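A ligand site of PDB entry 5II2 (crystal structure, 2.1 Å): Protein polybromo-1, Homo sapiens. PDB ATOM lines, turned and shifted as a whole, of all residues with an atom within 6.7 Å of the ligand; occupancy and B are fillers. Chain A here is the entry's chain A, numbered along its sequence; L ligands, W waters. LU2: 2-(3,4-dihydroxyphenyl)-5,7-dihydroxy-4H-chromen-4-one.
OH of Tyr 54 is in hydrogen-bond range of O2 of the ligand (2.6 Å).
The backbone carbonyl oxygen (O) of Phe 42 is in hydrogen-bond range of an oxygen (O1) of the ligand, at 2.7 Å.
The side-chain amide nitrogen (ND2) of Asn 97 is in hydrogen-bond range of an oxygen (O3) of the ligand.
The backbone NH (N) of Ala 93 sits close to an oxygen (O2) of the ligand (3.4 Å).
O1 of the ligand is in hydrogen-bond range of O of Met 62, at 3.4 Å.
The side-chain sulfur (SD) of Met 89 sits close to an oxygen (O1) of the ligand (3.6 Å).
O of Phe 42 lies within hydrogen-bond range of N of Met 64 (3.2 Å).
The side-chain amide nitrogen (ND2) of Asn 97 sits at hydrogen-bond distance from the backbone carbonyl oxygen (O) of Ala 93.
The side-chain carboxylate of Asp 63 sits at hydrogen-bond distance from the backbone NH of Leu 45, 2.8 Å away.
OD2 of Asp 63 lies within salt-bridge range of NH1 of Arg 44, 3.0 Å away.
SD of Met 89 sits close to N of Met 64.
An oxygen (O4) of the ligand sits close to the backbone carbonyl oxygen (O) of Ile 41, at 3.4 Å.
CD2 of Leu 45 touches C6 of the ligand, 3.6 Å away.
Pro 46 touches the ligand (CG to C15, 3.6 Å).
Leu 51 touches the ligand.
CB of Asp 63 touches O1 of the ligand, 3.4 Å away.
C of Asn 92 touches O2 of the ligand (3.8 Å).
Tyr 96 touches the ligand (CD2 to O3, 3.8 Å).
Ile 103 touches the ligand.
Of the 22 residues printed, 14 come within 4 Å of the ligand.
Along chain A the residues within 4 Å of the ligand span positions 41 to 103.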
ATOM      1  N   ILE A  41     -20.622  26.009  18.368  1.00  0.00           N
ATOM      2  CA  ILE A  41     -19.666  26.999  17.838  1.00  0.00           C
ATOM      3  C   ILE A  41     -20.089  27.585  16.474  1.00  0.00           C
ATOM      4  O   ILE A  41     -19.690  28.719  16.114  1.00  0.00           O
ATOM      5  CB  ILE A  41     -18.227  26.342  17.781  1.00  0.00           C
ATOM      6  CG1 ILE A  41     -17.122  27.339  17.978  1.00  0.00           C
ATOM      7  CG2 ILE A  41     -18.003  25.543  16.495  1.00  0.00           C
ATOM      8  CD1 ILE A  41     -15.756  26.706  18.061  1.00  0.00           C
ATOM      9  N   PHE A  42     -20.884  26.826  15.708  1.00  0.00           N
ATOM     10  CA  PHE A  42     -21.232  27.189  14.324  1.00  0.00           C
ATOM     11  C   PHE A  42     -22.407  28.146  14.192  1.00  0.00           C
ATOM     12  O   PHE A  42     -22.561  28.771  13.131  1.00  0.00           O
ATOM     13  CB  PHE A  42     -21.502  25.972  13.476  1.00  0.00           C
ATOM     14  CG  PHE A  42     -20.328  25.094  13.249  1.00  0.00           C
ATOM     15  CD1 PHE A  42     -19.446  25.349  12.191  1.00  0.00           C
ATOM     16  CD2 PHE A  42     -20.115  23.974  14.033  1.00  0.00           C
ATOM     17  CE1 PHE A  42     -18.370  24.512  11.964  1.00  0.00           C
ATOM     18  CE2 PHE A  42     -19.036  23.145  13.818  1.00  0.00           C
ATOM     19  CZ  PHE A  42     -18.153  23.409  12.763  1.00  0.00           C
ATOM     20  N   LEU A  43     -23.195  28.266  15.279  1.00  0.00           N
ATOM     21  CA  LEU A  43     -24.458  29.046  15.225  1.00  0.00           C
ATOM     22  C   LEU A  43     -24.279  30.495  14.708  1.00  0.00           C
ATOM     23  O   LEU A  43     -24.898  30.886  13.714  1.00  0.00           O
ATOM     24  CB  LEU A  43     -25.130  29.067  16.594  1.00  0.00           C
ATOM     25  CG  LEU A  43     -25.489  27.720  17.199  1.00  0.00           C
ATOM     26  CD1 LEU A  43     -26.279  27.917  18.536  1.00  0.00           C
ATOM     27  CD2 LEU A  43     -26.228  26.855  16.178  1.00  0.00           C
ATOM     28  N   ARG A  44     -23.328  31.211  15.323  1.00  0.00           N
ATOM     29  CA  ARG A  44     -23.016  32.570  14.977  1.00  0.00           C
ATOM     30  C   ARG A  44     -21.538  32.790  14.858  1.00  0.00           C
ATOM     31  O   ARG A  44     -20.790  32.617  15.848  1.00  0.00           O
ATOM     32  CB  ARG A  44     -23.598  33.549  16.029  1.00  0.00           C
ATOM     33  CG  ARG A  44     -23.591  34.966  15.592  1.00  0.00           C
ATOM     34  CD  ARG A  44     -24.544  35.286  14.416  1.00  0.00           C
ATOM     35  NE  ARG A  44     -24.482  36.722  14.097  1.00  0.00           N
ATOM     36  CZ  ARG A  44     -23.740  37.292  13.141  1.00  0.00           C
ATOM     37  NH1 ARG A  44     -23.052  36.576  12.259  1.00  0.00           N
ATOM     38  NH2 ARG A  44     -23.737  38.625  13.009  1.00  0.00           N
ATOM     39  N   LEU A  45     -21.133  33.213  13.655  1.00  0.00           N
ATOM     40  CA  LEU A  45     -19.725  33.599  13.386  1.00  0.00           C
ATOM     41  C   LEU A  45     -19.335  34.736  14.260  1.00  0.00           C
ATOM     42  O   LEU A  45     -20.119  35.685  14.411  1.00  0.00           O
ATOM     43  CB  LEU A  45     -19.521  34.067  11.947  1.00  0.00           C
ATOM     44  CG  LEU A  45     -19.001  33.014  11.015  1.00  0.00           C
ATOM     45  CD1 LEU A  45     -19.085  33.516   9.571  1.00  0.00           C
ATOM     46  CD2 LEU A  45     -17.583  32.618  11.365  1.00  0.00           C
ATOM     47  N   PRO A  46     -18.123  34.661  14.842  1.00  0.00           N
ATOM     48  CA  PRO A  46     -17.569  35.822  15.472  1.00  0.00           C
ATOM     49  C   PRO A  46     -17.242  36.909  14.458  1.00  0.00           C
ATOM     50  O   PRO A  46     -17.279  36.690  13.255  1.00  0.00           O
ATOM     51  CB  PRO A  46     -16.289  35.273  16.118  1.00  0.00           C
ATOM     52  CG  PRO A  46     -16.550  33.826  16.368  1.00  0.00           C
ATOM     53  CD  PRO A  46     -17.406  33.420  15.187  1.00  0.00           C
ATOM     54  N   GLU A  50     -12.549  39.425  16.172  1.00  0.00           N
ATOM     55  CA  GLU A  50     -12.511  38.256  16.988  1.00  0.00           C
ATOM     56  C   GLU A  50     -11.845  37.103  16.265  1.00  0.00           C
ATOM     57  O   GLU A  50     -11.265  36.218  16.939  1.00  0.00           O
ATOM     58  CB  GLU A  50     -13.946  37.909  17.451  1.00  0.00           C
ATOM     59  CG  GLU A  50     -14.493  38.922  18.457  1.00  0.00           C
ATOM     60  CD  GLU A  50     -15.967  38.675  18.786  1.00  0.00           C
ATOM     61  OE1 GLU A  50     -16.732  38.202  17.883  1.00  0.00           O
ATOM     62  OE2 GLU A  50     -16.387  38.929  19.942  1.00  0.00           O
ATOM     63  N   LEU A  51     -11.930  37.088  14.927  1.00  0.00           N
ATOM     64  CA  LEU A  51     -11.320  36.023  14.148  1.00  0.00           C
ATOM     65  C   LEU A  51     -10.326  36.599  13.089  1.00  0.00           C
ATOM     66  O   LEU A  51     -10.727  36.804  11.938  1.00  0.00           O
ATOM     67  CB  LEU A  51     -12.398  35.171  13.461  1.00  0.00           C
ATOM     68  CG  LEU A  51     -13.178  34.152  14.316  1.00  0.00           C
ATOM     69  CD1 LEU A  51     -14.155  33.367  13.461  1.00  0.00           C
ATOM     70  CD2 LEU A  51     -12.267  33.185  15.021  1.00  0.00           C
ATOM     71  N   TYR A  54     -10.247  36.082   8.978  1.00  0.00           N
ATOM     72  CA  TYR A  54     -11.375  35.282   8.517  1.00  0.00           C
ATOM     73  C   TYR A  54     -12.040  35.941   7.308  1.00  0.00           C
ATOM     74  O   TYR A  54     -12.159  35.340   6.254  1.00  0.00           O
ATOM     75  CB  TYR A  54     -12.410  35.082   9.607  1.00  0.00           C
ATOM     76  CG  TYR A  54     -13.384  33.970   9.260  1.00  0.00           C
ATOM     77  CD1 TYR A  54     -13.126  32.673   9.632  1.00  0.00           C
ATOM     78  CD2 TYR A  54     -14.568  34.218   8.575  1.00  0.00           C
ATOM     79  CE1 TYR A  54     -14.015  31.668   9.384  1.00  0.00           C
ATOM     80  CE2 TYR A  54     -15.463  33.207   8.273  1.00  0.00           C
ATOM     81  CZ  TYR A  54     -15.193  31.939   8.692  1.00  0.00           C
ATOM     82  OH  TYR A  54     -16.000  30.885   8.393  1.00  0.00           O
ATOM     83  N   ILE A  58     -12.084  34.225   3.787  1.00  0.00           N
ATOM     84  CA  ILE A  58     -13.277  33.470   3.468  1.00  0.00           C
ATOM     85  C   ILE A  58     -14.244  34.282   2.575  1.00  0.00           C
ATOM     86  O   ILE A  58     -14.851  35.240   3.029  1.00  0.00           O
ATOM     87  CB  ILE A  58     -13.981  32.990   4.775  1.00  0.00           C
ATOM     88  CG1 ILE A  58     -13.084  32.066   5.584  1.00  0.00           C
ATOM     89  CG2 ILE A  58     -15.303  32.306   4.465  1.00  0.00           C
ATOM     90  CD1 ILE A  58     -12.545  30.847   4.840  1.00  0.00           C
ATOM     91  N   MET A  62     -20.683  32.223   6.396  1.00  0.00           N
ATOM     92  CA  MET A  62     -21.907  31.528   6.572  1.00  0.00           C
ATOM     93  C   MET A  62     -21.942  30.981   7.956  1.00  0.00           C
ATOM     94  O   MET A  62     -20.955  30.418   8.433  1.00  0.00           O
ATOM     95  CB  MET A  62     -21.984  30.379   5.549  1.00  0.00           C
ATOM     96  CG  MET A  62     -23.316  29.644   5.500  1.00  0.00           C
ATOM     97  SD  MET A  62     -24.746  30.707   5.177  1.00  0.00           S
ATOM     98  CE  MET A  62     -24.353  31.292   3.533  1.00  0.00           C
ATOM     99  N   ASP A  63     -23.065  31.140   8.609  1.00  0.00           N
ATOM    100  CA  ASP A  63     -23.265  30.521   9.919  1.00  0.00           C
ATOM    101  C   ASP A  63     -24.673  30.004  10.020  1.00  0.00           C
ATOM    102  O   ASP A  63     -25.482  30.267   9.161  1.00  0.00           O
ATOM    103  CB  ASP A  63     -22.853  31.488  11.031  1.00  0.00           C
ATOM    104  CG  ASP A  63     -23.708  32.733  11.125  1.00  0.00           C
ATOM    105  OD1 ASP A  63     -24.816  32.789  10.535  1.00  0.00           O
ATOM    106  OD2 ASP A  63     -23.214  33.662  11.808  1.00  0.00           O
ATOM    107  N   MET A  64     -24.959  29.217  11.039  1.00  0.00           N
ATOM    108  CA  MET A  64     -26.257  28.597  11.097  1.00  0.00           C
ATOM    109  C   MET A  64     -27.375  29.597  11.296  1.00  0.00           C
ATOM    110  O   MET A  64     -28.476  29.322  10.852  1.00  0.00           O
ATOM    111  CB  MET A  64     -26.296  27.467  12.114  1.00  0.00           C
ATOM    112  CG  MET A  64     -25.477  26.284  11.646  1.00  0.00           C
ATOM    113  SD  MET A  64     -25.520  24.839  12.675  1.00  0.00           S
ATOM    114  CE  MET A  64     -27.242  24.438  12.738  1.00  0.00           C
ATOM    115  N   MET A  89     -20.502  26.518   4.883  1.00  0.00           N
ATOM    116  CA  MET A  89     -20.055  26.739   6.256  1.00  0.00           C
ATOM    117  C   MET A  89     -18.967  25.765   6.717  1.00  0.00           C
ATOM    118  O   MET A  89     -17.946  26.166   7.309  1.00  0.00           O
ATOM    119  CB  MET A  89     -21.251  26.704   7.238  1.00  0.00           C
ATOM    120  CG  MET A  89     -20.983  27.158   8.670  1.00  0.00           C
ATOM    121  SD  MET A  89     -22.445  26.852   9.741  1.00  0.00           S
ATOM    122  CE  MET A  89     -22.568  25.069   9.776  1.00  0.00           C
ATOM    123  N   PHE A  90     -19.201  24.492   6.484  1.00  0.00           N
ATOM    124  CA  PHE A  90     -18.243  23.474   6.920  1.00  0.00           C
ATOM    125  C   PHE A  90     -16.899  23.686   6.156  1.00  0.00           C
ATOM    126  O   PHE A  90     -15.835  23.654   6.777  1.00  0.00           O
ATOM    127  CB  PHE A  90     -18.798  22.065   6.701  1.00  0.00           C
ATOM    128  CG  PHE A  90     -20.073  21.761   7.493  1.00  0.00           C
ATOM    129  CD1 PHE A  90     -20.222  22.136   8.811  1.00  0.00           C
ATOM    130  CD2 PHE A  90     -21.112  21.070   6.902  1.00  0.00           C
ATOM    131  CE1 PHE A  90     -21.363  21.841   9.529  1.00  0.00           C
ATOM    132  CE2 PHE A  90     -22.244  20.757   7.612  1.00  0.00           C
ATOM    133  CZ  PHE A  90     -22.359  21.138   8.942  1.00  0.00           C
ATOM    134  N   ASN A  91     -16.959  23.910   4.856  1.00  0.00           N
ATOM    135  CA  ASN A  91     -15.732  24.200   4.076  1.00  0.00           C
ATOM    136  C   ASN A  91     -14.986  25.459   4.572  1.00  0.00           C
ATOM    137  O   ASN A  91     -13.741  25.466   4.632  1.00  0.00           O
ATOM    138  CB  ASN A  91     -15.994  24.327   2.607  1.00  0.00           C
ATOM    139  CG  ASN A  91     -15.919  23.006   1.900  1.00  0.00           C
ATOM    140  OD1 ASN A  91     -14.977  22.219   2.101  1.00  0.00           O
ATOM    141  ND2 ASN A  91     -16.906  22.751   1.044  1.00  0.00           N
ATOM    142  N   ASN A  92     -15.737  26.480   4.949  1.00  0.00           N
ATOM    143  CA  ASN A  92     -15.169  27.693   5.502  1.00  0.00           C
ATOM    144  C   ASN A  92     -14.413  27.384   6.758  1.00  0.00           C
ATOM    145  O   ASN A  92     -13.285  27.809   6.885  1.00  0.00           O
ATOM    146  CB  ASN A  92     -16.206  28.745   5.776  1.00  0.00           C
ATOM    147  CG  ASN A  92     -16.772  29.341   4.527  1.00  0.00           C
ATOM    148  OD1 ASN A  92     -16.197  29.216   3.465  1.00  0.00           O
ATOM    149  ND2 ASN A  92     -17.902  30.013   4.639  1.00  0.00           N
ATOM    150  N   ALA A  93     -15.011  26.602   7.652  1.00  0.00           N
ATOM    151  CA  ALA A  93     -14.413  26.276   8.899  1.00  0.00           C
ATOM    152  C   ALA A  93     -13.173  25.431   8.660  1.00  0.00           C
ATOM    153  O   ALA A  93     -12.165  25.587   9.351  1.00  0.00           O
ATOM    154  CB  ALA A  93     -15.448  25.551   9.822  1.00  0.00           C
ATOM    155  N   CYS A  94     -13.270  24.524   7.700  1.00  0.00           N
ATOM    156  CA  CYS A  94     -12.151  23.693   7.341  1.00  0.00           C
ATOM    157  C   CYS A  94     -11.065  24.471   6.601  1.00  0.00           C
ATOM    158  O   CYS A  94      -9.941  24.178   6.770  1.00  0.00           O
ATOM    159  CB  CYS A  94     -12.568  22.431   6.583  1.00  0.00           C
ATOM    160  SG  CYS A  94     -13.451  21.292   7.689  1.00  0.00           S
ATOM    161  N   TYR A  96     -10.386  27.828   7.277  1.00  0.00           N
ATOM    162  CA  TYR A  96      -9.774  28.656   8.285  1.00  0.00           C
ATOM    163  C   TYR A  96      -8.995  27.945   9.378  1.00  0.00           C
ATOM    164  O   TYR A  96      -8.034  28.496   9.879  1.00  0.00           O
ATOM    165  CB  TYR A  96     -10.825  29.472   8.999  1.00  0.00           C
ATOM    166  CG  TYR A  96     -10.322  30.571   9.857  1.00  0.00           C
ATOM    167  CD1 TYR A  96      -9.656  31.674   9.302  1.00  0.00           C
ATOM    168  CD2 TYR A  96     -10.558  30.565  11.239  1.00  0.00           C
ATOM    169  CE1 TYR A  96      -9.210  32.707  10.095  1.00  0.00           C
ATOM    170  CE2 TYR A  96     -10.153  31.627  12.043  1.00  0.00           C
ATOM    171  CZ  TYR A  96      -9.509  32.692  11.474  1.00  0.00           C
ATOM    172  OH  TYR A  96      -9.105  33.717  12.301  1.00  0.00           O
ATOM    173  N   ASN A  97      -9.477  26.784   9.801  1.00  0.00           N
ATOM    174  CA  ASN A  97      -8.878  26.098  10.960  1.00  0.00           C
ATOM    175  C   ASN A  97      -8.055  24.931  10.507  1.00  0.00           C
ATOM    176  O   ASN A  97      -8.168  24.476   9.340  1.00  0.00           O
ATOM    177  CB  ASN A  97      -9.989  25.617  11.867  1.00  0.00           C
ATOM    178  CG  ASN A  97     -10.813  26.776  12.383  1.00  0.00           C
ATOM    179  OD1 ASN A  97     -10.407  27.418  13.321  1.00  0.00           O
ATOM    180  ND2 ASN A  97     -11.960  27.059  11.761  1.00  0.00           N
ATOM    181  N   ILE A 103     -13.005  22.307  15.891  1.00  0.00           N
ATOM    182  CA  ILE A 103     -13.993  22.830  14.957  1.00  0.00           C
ATOM    183  C   ILE A 103     -13.923  22.085  13.595  1.00  0.00           C
ATOM    184  O   ILE A 103     -14.936  21.658  13.058  1.00  0.00           O
ATOM    185  CB  ILE A 103     -13.926  24.383  14.854  1.00  0.00           C
ATOM    186  CG1 ILE A 103     -15.167  24.882  14.051  1.00  0.00           C
ATOM    187  CG2 ILE A 103     -12.642  24.835  14.199  1.00  0.00           C
ATOM    188  CD1 ILE A 103     -15.385  26.341  13.918  1.00  0.00           C
HETATM  189  C1  LU2 L   1     -18.609  29.577  13.090  1.00  0.00           C
HETATM  190  O1  LU2 L   1     -20.392  29.258  11.541  1.00  0.00           O
HETATM  191  C2  LU2 L   1     -19.057  29.293  11.797  1.00  0.00           C
HETATM  192  O2  LU2 L   1     -15.837  28.880   9.982  1.00  0.00           O
HETATM  193  C3  LU2 L   1     -18.136  29.060  10.776  1.00  0.00           C
HETATM  194  O3  LU2 L   1     -14.052  29.136  11.763  1.00  0.00           O
HETATM  195  C4  LU2 L   1     -16.744  29.099  11.015  1.00  0.00           C
HETATM  196  O4  LU2 L   1     -16.848  29.925  14.610  1.00  0.00           O
HETATM  197  C5  LU2 L   1     -16.283  29.382  12.314  1.00  0.00           C
HETATM  198  O5  LU2 L   1     -12.305  30.166  18.637  1.00  0.00           O
HETATM  199  C6  LU2 L   1     -17.236  29.624  13.337  1.00  0.00           C
HETATM  200  O6  LU2 L   1     -14.402  30.684  20.342  1.00  0.00           O
HETATM  201  C7  LU2 L   1     -14.904  29.425  12.613  1.00  0.00           C
HETATM  202  C8  LU2 L   1     -14.524  29.648  13.943  1.00  0.00           C
HETATM  203  C9  LU2 L   1     -15.501  29.922  14.929  1.00  0.00           C
HETATM  204  C10 LU2 L   1     -15.175  30.137  16.286  1.00  0.00           C
HETATM  205  C11 LU2 L   1     -13.841  30.044  16.779  1.00  0.00           C
HETATM  206  C12 LU2 L   1     -13.585  30.238  18.142  1.00  0.00           C
HETATM  207  C13 LU2 L   1     -14.647  30.500  19.021  1.00  0.00           C
HETATM  208  C14 LU2 L   1     -15.955  30.618  18.548  1.00  0.00           C
HETATM  209  C15 LU2 L   1     -16.203  30.388  17.205  1.00  0.00           C
HETATM  210  O   HOH W   1     -11.087  29.362  15.053  1.00  0.00           O
HETATM  211  O   HOH W   2     -11.514  27.613  17.418  1.00  0.00           O
HETATM  212  O   HOH W   3     -15.992  31.098  22.341  1.00  0.00           O
HETATM  213  O   HOH W   4     -10.806  30.663  21.015  1.00  0.00           O
